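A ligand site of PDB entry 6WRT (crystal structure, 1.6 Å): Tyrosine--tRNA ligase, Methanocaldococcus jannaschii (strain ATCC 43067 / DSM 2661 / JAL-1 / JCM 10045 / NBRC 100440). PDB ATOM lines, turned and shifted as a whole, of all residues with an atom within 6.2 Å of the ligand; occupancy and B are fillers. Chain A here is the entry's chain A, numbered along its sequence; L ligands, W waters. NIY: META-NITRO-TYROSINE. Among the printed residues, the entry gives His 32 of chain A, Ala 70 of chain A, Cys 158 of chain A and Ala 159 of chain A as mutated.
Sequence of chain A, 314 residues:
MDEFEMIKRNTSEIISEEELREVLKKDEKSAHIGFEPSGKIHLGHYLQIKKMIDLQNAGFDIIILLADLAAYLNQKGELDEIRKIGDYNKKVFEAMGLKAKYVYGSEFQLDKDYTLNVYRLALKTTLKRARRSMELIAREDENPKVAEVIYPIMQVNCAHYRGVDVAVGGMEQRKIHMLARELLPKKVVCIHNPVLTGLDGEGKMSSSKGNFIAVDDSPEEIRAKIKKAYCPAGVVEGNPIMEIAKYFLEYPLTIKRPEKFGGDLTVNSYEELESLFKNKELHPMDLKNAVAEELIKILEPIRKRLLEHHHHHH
OE1 of Gln 173 sits at hydrogen-bond distance from N of the ligand (2.8 Å). A nitrogen (N) of the ligand sits at hydrogen-bond distance from the side-chain hydroxyl (OH) of Tyr 151 (2.8 Å). The side-chain amide oxygen (OE1) of Gln 155 lies within hydrogen-bond range of a nitrogen (N) of the ligand, at 2.8 Å. The side-chain amide nitrogen (NE2) of Gln 109 lies within hydrogen-bond range of an oxygen (O2) of the ligand (2.9 Å). The backbone NH (N) of Glu 36 sits at hydrogen-bond distance from an oxygen (OXT) of the ligand, at 3.0 Å. The side-chain sulfur of Cys 158 lies close to an oxygen (OH) of the ligand (3.3 Å).
The side-chain amide oxygen (OE1) of Gln 173 is in hydrogen-bond range of the side-chain amide nitrogen (NE2) of Gln 155 (3.0 Å). The side-chain amide nitrogen (NE2) of Gln 173 sits at hydrogen-bond distance from the side-chain carboxylate (OE2) of Glu 172, 2.9 Å away. OH of Tyr 151 is in hydrogen-bond range of OE2 of Glu 36. OE1 of Gln 109 sits close to O of Gly 105, at 3.5 Å. N of Cys 158 sits at hydrogen-bond distance from OH of Tyr 114 (3.1 Å). The backbone NH (N) of Phe 35 is in hydrogen-bond range of the backbone carbonyl oxygen (O) of Leu 65. The backbone carbonyl oxygen of Ile 33 sits at hydrogen-bond distance from the backbone NH of Leu 65 (2.8 Å). The backbone carbonyl oxygen (O) of Phe 35 is in hydrogen-bond range of the backbone NH (N) of Ala 67 (2.9 Å).
Merely in contact with the ligand: Gly 34 (3.4 Å), Ala 70 (3.4 Å), Leu 65 (3.5 Å), Ala 67 (3.5 Å), Phe 35 (3.7 Å) and Met 154 (3.8 Å). Hydrophobic or aromatic side chains within 4 Å of the ligand: Leu 65, Ala 67, Ala 70 and Tyr 151. Of the 24 residues printed, 12 come within 4 Å of the ligand.
Water W4 lies within hydrogen-bond range of OE1 of Gln 109 (2.7 Å), N of Ala 70 (2.9 Å), O1 of the ligand (3.0 Å) and N of Leu 69 (3.3 Å). Water W2 lies within hydrogen-bond range of NE2 of His 177 (2.7 Å) and NE2 of Gln 155 (3.4 Å).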
ATOM      1  N   HIS A  32      -6.401  23.326  10.971  1.00  0.00           N
ATOM      2  CA  HIS A  32      -5.434  22.417  11.574  1.00  0.00           C
ATOM      3  C   HIS A  32      -4.914  21.357  10.629  1.00  0.00           C
ATOM      4  O   HIS A  32      -5.486  21.121   9.625  1.00  0.00           O
ATOM      5  CB  HIS A  32      -5.895  21.813  12.930  1.00  0.00           C
ATOM      6  CG  HIS A  32      -6.726  20.562  12.856  1.00  0.00           C
ATOM      7  ND1 HIS A  32      -7.354  20.048  13.963  1.00  0.00           N
ATOM      8  CD2 HIS A  32      -6.985  19.696  11.854  1.00  0.00           C
ATOM      9  CE1 HIS A  32      -7.990  18.941  13.638  1.00  0.00           C
ATOM     10  NE2 HIS A  32      -7.788  18.713  12.360  1.00  0.00           N
ATOM     11  N   ILE A  33      -3.744  20.848  10.930  1.00  0.00           N
ATOM     12  CA  ILE A  33      -3.189  19.722  10.211  1.00  0.00           C
ATOM     13  C   ILE A  33      -2.524  18.845  11.256  1.00  0.00           C
ATOM     14  O   ILE A  33      -1.961  19.345  12.240  1.00  0.00           O
ATOM     15  CB  ILE A  33      -2.190  20.183   9.150  1.00  0.00           C
ATOM     16  CG1 ILE A  33      -1.547  19.005   8.456  1.00  0.00           C
ATOM     17  CG2 ILE A  33      -1.058  21.055   9.765  1.00  0.00           C
ATOM     18  CD1 ILE A  33      -0.977  19.356   7.094  1.00  0.00           C
ATOM     19  N   GLY A  34      -2.590  17.543  11.045  1.00  0.00           N
ATOM     20  CA  GLY A  34      -1.942  16.574  11.914  1.00  0.00           C
ATOM     21  C   GLY A  34      -0.807  15.886  11.185  1.00  0.00           C
ATOM     22  O   GLY A  34      -0.921  15.572   9.976  1.00  0.00           O
ATOM     23  N   PHE A  35       0.266  15.638  11.920  1.00  0.00           N
ATOM     24  CA  PHE A  35       1.385  14.882  11.394  1.00  0.00           C
ATOM     25  C   PHE A  35       1.763  13.786  12.383  1.00  0.00           C
ATOM     26  O   PHE A  35       2.040  14.069  13.559  1.00  0.00           O
ATOM     27  CB  PHE A  35       2.663  15.710  11.183  1.00  0.00           C
ATOM     28  CG  PHE A  35       2.556  16.838  10.191  1.00  0.00           C
ATOM     29  CD1 PHE A  35       2.639  16.610   8.830  1.00  0.00           C
ATOM     30  CD2 PHE A  35       2.421  18.145  10.663  1.00  0.00           C
ATOM     31  CE1 PHE A  35       2.594  17.679   7.948  1.00  0.00           C
ATOM     32  CE2 PHE A  35       2.379  19.212   9.789  1.00  0.00           C
ATOM     33  CZ  PHE A  35       2.461  18.970   8.438  1.00  0.00           C
ATOM     34  N   GLU A  36       1.817  12.537  11.917  1.00  0.00           N
ATOM     35  CA  GLU A  36       2.557  11.523  12.659  1.00  0.00           C
ATOM     36  C   GLU A  36       3.995  12.000  12.810  1.00  0.00           C
ATOM     37  O   GLU A  36       4.629  12.379  11.815  1.00  0.00           O
ATOM     38  CB  GLU A  36       2.548  10.202  11.908  1.00  0.00           C
ATOM     39  CG  GLU A  36       1.155   9.534  11.847  1.00  0.00           C
ATOM     40  CD  GLU A  36       1.215   8.122  11.252  1.00  0.00           C
ATOM     41  OE1 GLU A  36       2.212   7.431  11.513  1.00  0.00           O
ATOM     42  OE2 GLU A  36       0.262   7.708  10.546  1.00  0.00           O
ATOM     43  N   LEU A  65      -1.280  19.605  14.949  1.00  0.00           N
ATOM     44  CA  LEU A  65      -1.447  18.400  15.768  1.00  0.00           C
ATOM     45  C   LEU A  65      -0.208  17.510  15.601  1.00  0.00           C
ATOM     46  O   LEU A  65       0.116  17.063  14.499  1.00  0.00           O
ATOM     47  CB  LEU A  65      -2.720  17.656  15.351  1.00  0.00           C
ATOM     48  CG  LEU A  65      -2.966  16.358  16.082  1.00  0.00           C
ATOM     49  CD1 LEU A  65      -3.238  16.693  17.570  1.00  0.00           C
ATOM     50  CD2 LEU A  65      -4.136  15.580  15.514  1.00  0.00           C
ATOM     51  N   ALA A  67       0.671  14.131  16.093  1.00  0.00           N
ATOM     52  CA  ALA A  67      -0.309  13.035  16.191  1.00  0.00           C
ATOM     53  C   ALA A  67       0.361  11.789  16.760  1.00  0.00           C
ATOM     54  O   ALA A  67       0.627  10.778  16.079  1.00  0.00           O
ATOM     55  CB  ALA A  67      -0.949  12.811  14.827  1.00  0.00           C
ATOM     56  N   LEU A  69      -0.644   9.704  19.188  1.00  0.00           N
ATOM     57  CA  LEU A  69      -1.482   8.515  19.382  1.00  0.00           C
ATOM     58  C   LEU A  69      -1.763   7.840  17.980  1.00  0.00           C
ATOM     59  O   LEU A  69      -1.770   6.661  17.836  1.00  0.00           O
ATOM     60  CB  LEU A  69      -2.799   8.803  20.134  1.00  0.00           C
ATOM     61  CG  LEU A  69      -3.670   7.621  20.515  1.00  0.00           C
ATOM     62  CD1 LEU A  69      -2.901   6.631  21.377  1.00  0.00           C
ATOM     63  CD2 LEU A  69      -4.959   8.079  21.200  1.00  0.00           C
ATOM     64  N   ALA A  70      -2.100   8.649  16.974  1.00  0.00           N
ATOM     65  CA  ALA A  70      -2.236   8.083  15.604  1.00  0.00           C
ATOM     66  C   ALA A  70      -0.907   7.323  15.224  1.00  0.00           C
ATOM     67  O   ALA A  70      -0.949   6.264  14.687  1.00  0.00           O
ATOM     68  CB  ALA A  70      -2.506   9.129  14.493  1.00  0.00           C
ATOM     69  N   GLY A 105      -1.871  14.780  20.176  1.00  0.00           N
ATOM     70  CA  GLY A 105      -3.156  14.098  20.148  1.00  0.00           C
ATOM     71  C   GLY A 105      -3.542  13.523  21.489  1.00  0.00           C
ATOM     72  O   GLY A 105      -4.697  13.645  21.923  1.00  0.00           O
ATOM     73  N   PHE A 108      -5.878  14.961  24.421  1.00  0.00           N
ATOM     74  CA  PHE A 108      -7.335  14.975  24.420  1.00  0.00           C
ATOM     75  C   PHE A 108      -7.963  13.716  23.848  1.00  0.00           C
ATOM     76  O   PHE A 108      -9.151  13.467  24.101  1.00  0.00           O
ATOM     77  CB  PHE A 108      -7.872  16.195  23.668  1.00  0.00           C
ATOM     78  CG  PHE A 108      -7.433  16.267  22.227  1.00  0.00           C
ATOM     79  CD1 PHE A 108      -6.263  16.972  21.871  1.00  0.00           C
ATOM     80  CD2 PHE A 108      -8.191  15.703  21.224  1.00  0.00           C
ATOM     81  CE1 PHE A 108      -5.860  17.042  20.562  1.00  0.00           C
ATOM     82  CE2 PHE A 108      -7.777  15.791  19.902  1.00  0.00           C
ATOM     83  CZ  PHE A 108      -6.594  16.438  19.578  1.00  0.00           C
ATOM     84  N   GLN A 109      -7.198  12.939  23.122  1.00  0.00           N
ATOM     85  CA  GLN A 109      -7.792  11.790  22.420  1.00  0.00           C
ATOM     86  C   GLN A 109      -8.119  10.562  23.276  1.00  0.00           C
ATOM     87  O   GLN A 109      -8.648   9.587  22.795  1.00  0.00           O
ATOM     88  CB  GLN A 109      -6.978  11.360  21.165  1.00  0.00           C
ATOM     89  CG  GLN A 109      -6.891  12.442  20.115  1.00  0.00           C
ATOM     90  CD  GLN A 109      -5.987  12.038  18.926  1.00  0.00           C
ATOM     91  OE1 GLN A 109      -4.917  11.568  19.152  1.00  0.00           O
ATOM     92  NE2 GLN A 109      -6.427  12.221  17.705  1.00  0.00           N
ATOM     93  N   TYR A 114     -14.255  11.799  24.161  1.00  0.00           N
ATOM     94  CA  TYR A 114     -13.594  11.554  22.867  1.00  0.00           C
ATOM     95  C   TYR A 114     -13.795  10.004  22.540  1.00  0.00           C
ATOM     96  O   TYR A 114     -14.235   9.627  21.502  1.00  0.00           O
ATOM     97  CB  TYR A 114     -12.023  11.845  22.860  1.00  0.00           C
ATOM     98  CG  TYR A 114     -11.421  11.974  21.471  1.00  0.00           C
ATOM     99  CD1 TYR A 114     -11.088  10.871  20.732  1.00  0.00           C
ATOM    100  CD2 TYR A 114     -11.205  13.209  20.906  1.00  0.00           C
ATOM    101  CE1 TYR A 114     -10.552  10.981  19.495  1.00  0.00           C
ATOM    102  CE2 TYR A 114     -10.676  13.345  19.685  1.00  0.00           C
ATOM    103  CZ  TYR A 114     -10.336  12.232  18.954  1.00  0.00           C
ATOM    104  OH  TYR A 114      -9.785  12.381  17.715  1.00  0.00           O
ATOM    105  N   ILE A 137      -1.819   5.355   3.932  1.00  0.00           N
ATOM    106  CA  ILE A 137      -1.323   5.819   5.218  1.00  0.00           C
ATOM    107  C   ILE A 137      -0.765   4.686   6.047  1.00  0.00           C
ATOM    108  O   ILE A 137       0.254   4.851   6.754  1.00  0.00           O
ATOM    109  CB  ILE A 137      -2.475   6.523   5.987  1.00  0.00           C
ATOM    110  CG1 ILE A 137      -2.899   7.812   5.253  1.00  0.00           C
ATOM    111  CG2 ILE A 137      -2.060   6.836   7.415  1.00  0.00           C
ATOM    112  CD1 ILE A 137      -4.224   8.383   5.739  1.00  0.00           C
ATOM    113  N   TYR A 151      -7.530   3.930  13.781  1.00  0.00           N
ATOM    114  CA  TYR A 151      -6.856   5.144  13.297  1.00  0.00           C
ATOM    115  C   TYR A 151      -7.763   6.113  12.539  1.00  0.00           C
ATOM    116  O   TYR A 151      -7.867   7.279  12.917  1.00  0.00           O
ATOM    117  CB  TYR A 151      -5.662   4.727  12.448  1.00  0.00           C
ATOM    118  CG  TYR A 151      -4.727   5.800  11.944  1.00  0.00           C
ATOM    119  CD1 TYR A 151      -5.140   6.729  11.003  1.00  0.00           C
ATOM    120  CD2 TYR A 151      -3.419   5.861  12.388  1.00  0.00           C
ATOM    121  CE1 TYR A 151      -4.264   7.712  10.512  1.00  0.00           C
ATOM    122  CE2 TYR A 151      -2.536   6.818  11.880  1.00  0.00           C
ATOM    123  CZ  TYR A 151      -2.972   7.735  10.957  1.00  0.00           C
ATOM    124  OH  TYR A 151      -2.112   8.708  10.439  1.00  0.00           O
ATOM    125  N   MET A 154     -10.465   7.717  14.553  1.00  0.00           N
ATOM    126  CA  MET A 154      -9.820   8.611  15.518  1.00  0.00           C
ATOM    127  C   MET A 154      -9.599   9.999  14.829  1.00  0.00           C
ATOM    128  O   MET A 154      -9.777  11.021  15.413  1.00  0.00           O
ATOM    129  CB  MET A 154      -8.447   8.096  16.043  1.00  0.00           C
ATOM    130  CG  MET A 154      -7.653   9.037  16.903  1.00  0.00           C
ATOM    131  SD  MET A 154      -6.746   8.130  18.153  1.00  0.00           S
ATOM    132  CE  MET A 154      -8.253   7.438  18.887  1.00  0.00           C
ATOM    133  N   GLN A 155      -9.097   9.985  13.602  1.00  0.00           N
ATOM    134  CA  GLN A 155      -8.852  11.222  12.853  1.00  0.00           C
ATOM    135  C   GLN A 155     -10.169  11.920  12.500  1.00  0.00           C
ATOM    136  O   GLN A 155     -10.253  13.159  12.621  1.00  0.00           O
ATOM    137  CB  GLN A 155      -8.007  10.910  11.611  1.00  0.00           C
ATOM    138  CG  GLN A 155      -7.741  12.094  10.752  1.00  0.00           C
ATOM    139  CD  GLN A 155      -6.575  11.837   9.792  1.00  0.00           C
ATOM    140  OE1 GLN A 155      -5.806  10.909  10.016  1.00  0.00           O
ATOM    141  NE2 GLN A 155      -6.483  12.624   8.706  1.00  0.00           N
ATOM    142  N   VAL A 156     -11.209  11.169  12.187  1.00  0.00           N
ATOM    143  CA  VAL A 156     -12.535  11.754  11.965  1.00  0.00           C
ATOM    144  C   VAL A 156     -12.990  12.501  13.205  1.00  0.00           C
ATOM    145  O   VAL A 156     -13.482  13.642  13.136  1.00  0.00           O
ATOM    146  CB  VAL A 156     -13.527  10.663  11.551  1.00  0.00           C
ATOM    147  CG1 VAL A 156     -14.981  11.224  11.633  1.00  0.00           C
ATOM    148  CG2 VAL A 156     -13.209  10.075  10.177  1.00  0.00           C
ATOM    149  N   CYS A 158     -11.285  13.799  15.459  1.00  0.00           N
ATOM    150  CA  CYS A 158     -10.410  14.900  15.843  1.00  0.00           C
ATOM    151  C   CYS A 158     -10.950  16.286  15.336  1.00  0.00           C
ATOM    152  O   CYS A 158     -11.096  17.241  16.062  1.00  0.00           O
ATOM    153  CB  CYS A 158      -8.949  14.681  15.409  1.00  0.00           C
ATOM    154  SG  CYS A 158      -7.856  15.915  16.006  1.00  0.00           S
ATOM    155  N   ALA A 159     -11.223  16.381  14.052  1.00  0.00           N
ATOM    156  CA  ALA A 159     -11.778  17.649  13.516  1.00  0.00           C
ATOM    157  C   ALA A 159     -13.135  17.946  14.263  1.00  0.00           C
ATOM    158  O   ALA A 159     -13.417  19.061  14.553  1.00  0.00           O
ATOM    159  CB  ALA A 159     -12.031  17.678  12.001  1.00  0.00           C
ATOM    160  N   GLU A 172      -3.268  11.913   0.406  1.00  0.00           N
ATOM    161  CA  GLU A 172      -3.363  10.600   1.023  1.00  0.00           C
ATOM    162  C   GLU A 172      -4.402  10.566   2.149  1.00  0.00           C
ATOM    163  O   GLU A 172      -4.778   9.478   2.599  1.00  0.00           O
ATOM    164  CB  GLU A 172      -2.001  10.144   1.559  1.00  0.00           C
ATOM    165  CG  GLU A 172      -1.529  10.827   2.857  1.00  0.00           C
ATOM    166  CD  GLU A 172      -0.948  12.223   2.645  1.00  0.00           C
ATOM    167  OE1 GLU A 172      -0.600  12.561   1.495  1.00  0.00           O
ATOM    168  OE2 GLU A 172      -0.821  12.976   3.652  1.00  0.00           O
ATOM    169  N   GLN A 173      -4.824  11.725   2.627  1.00  0.00           N
ATOM    170  CA  GLN A 173      -5.800  11.839   3.692  1.00  0.00           C
ATOM    171  C   GLN A 173      -7.238  11.958   3.168  1.00  0.00           C
ATOM    172  O   GLN A 173      -8.176  12.006   3.984  1.00  0.00           O
ATOM    173  CB  GLN A 173      -5.539  13.095   4.533  1.00  0.00           C
ATOM    174  CG  GLN A 173      -4.097  13.296   5.049  1.00  0.00           C
ATOM    175  CD  GLN A 173      -3.638  12.185   5.952  1.00  0.00           C
ATOM    176  OE1 GLN A 173      -4.320  11.784   6.877  1.00  0.00           O
ATOM    177  NE2 GLN A 173      -2.415  11.736   5.702  1.00  0.00           N
ATOM    178  N   ILE A 176     -10.132   9.554   4.397  1.00  0.00           N
ATOM    179  CA  ILE A 176     -10.507   9.798   5.796  1.00  0.00           C
ATOM    180  C   ILE A 176     -11.339  11.075   5.916  1.00  0.00           C
ATOM    181  O   ILE A 176     -12.352  11.119   6.642  1.00  0.00           O
ATOM    182  CB  ILE A 176      -9.257   9.875   6.705  1.00  0.00           C
ATOM    183  CG1 ILE A 176      -8.566   8.529   6.792  1.00  0.00           C
ATOM    184  CG2 ILE A 176      -9.653  10.426   8.072  1.00  0.00           C
ATOM    185  CD1 ILE A 176      -7.264   8.562   7.557  1.00  0.00           C
ATOM    186  N   HIS A 177     -10.948  12.135   5.167  1.00  0.00           N
ATOM    187  CA  HIS A 177     -11.676  13.396   5.235  1.00  0.00           C
ATOM    188  C   HIS A 177     -13.076  13.260   4.657  1.00  0.00           C
ATOM    189  O   HIS A 177     -14.026  13.822   5.192  1.00  0.00           O
ATOM    190  CB  HIS A 177     -10.873  14.485   4.526  1.00  0.00           C
ATOM    191  CG  HIS A 177      -9.708  14.961   5.330  1.00  0.00           C
ATOM    192  ND1 HIS A 177      -8.699  15.741   4.797  1.00  0.00           N
ATOM    193  CD2 HIS A 177      -9.359  14.728   6.623  1.00  0.00           C
ATOM    194  CE1 HIS A 177      -7.839  16.029   5.740  1.00  0.00           C
ATOM    195  NE2 HIS A 177      -8.194  15.415   6.849  1.00  0.00           N
HETATM  196  N   NIY L   1      -3.136  10.972   9.228  1.00  0.00           N
HETATM  197  CA  NIY L   1      -2.069  11.955   9.482  1.00  0.00           C
HETATM  198  C   NIY L   1      -0.731  11.520   8.909  1.00  0.00           C
HETATM  199  O   NIY L   1      -0.754  10.713   8.007  1.00  0.00           O
HETATM  200  CB  NIY L   1      -1.969  12.227  10.972  1.00  0.00           C
HETATM  201  CG  NIY L   1      -3.235  12.833  11.579  1.00  0.00           C
HETATM  202  CD1 NIY L   1      -3.770  12.328  12.738  1.00  0.00           C
HETATM  203  CD2 NIY L   1      -3.814  13.918  11.000  1.00  0.00           C
HETATM  204  CE1 NIY L   1      -4.885  12.899  13.306  1.00  0.00           C
HETATM  205  CE2 NIY L   1      -4.917  14.513  11.533  1.00  0.00           C
HETATM  206  CZ  NIY L   1      -5.473  14.009  12.700  1.00  0.00           C
HETATM  207  OH  NIY L   1      -6.567  14.571  13.248  1.00  0.00           O
HETATM  208  NN  NIY L   1      -5.408  12.359  14.488  1.00  0.00           N
HETATM  209  O1  NIY L   1      -4.861  11.536  15.110  1.00  0.00           O
HETATM  210  O2  NIY L   1      -6.446  12.705  14.849  1.00  0.00           O
HETATM  211  OXT NIY L   1       0.301  11.974   9.353  1.00  0.00           O
HETATM  212  O   HOH W   1       2.372  12.670   7.844  1.00  0.00           O
HETATM  213  O   HOH W   2      -7.046  15.947   9.228  1.00  0.00           O
HETATM  214  O   HOH W   3       1.063   9.400   6.569  1.00  0.00           O
HETATM  215  O   HOH W   4      -2.837  11.426  17.382  1.00  0.00           O
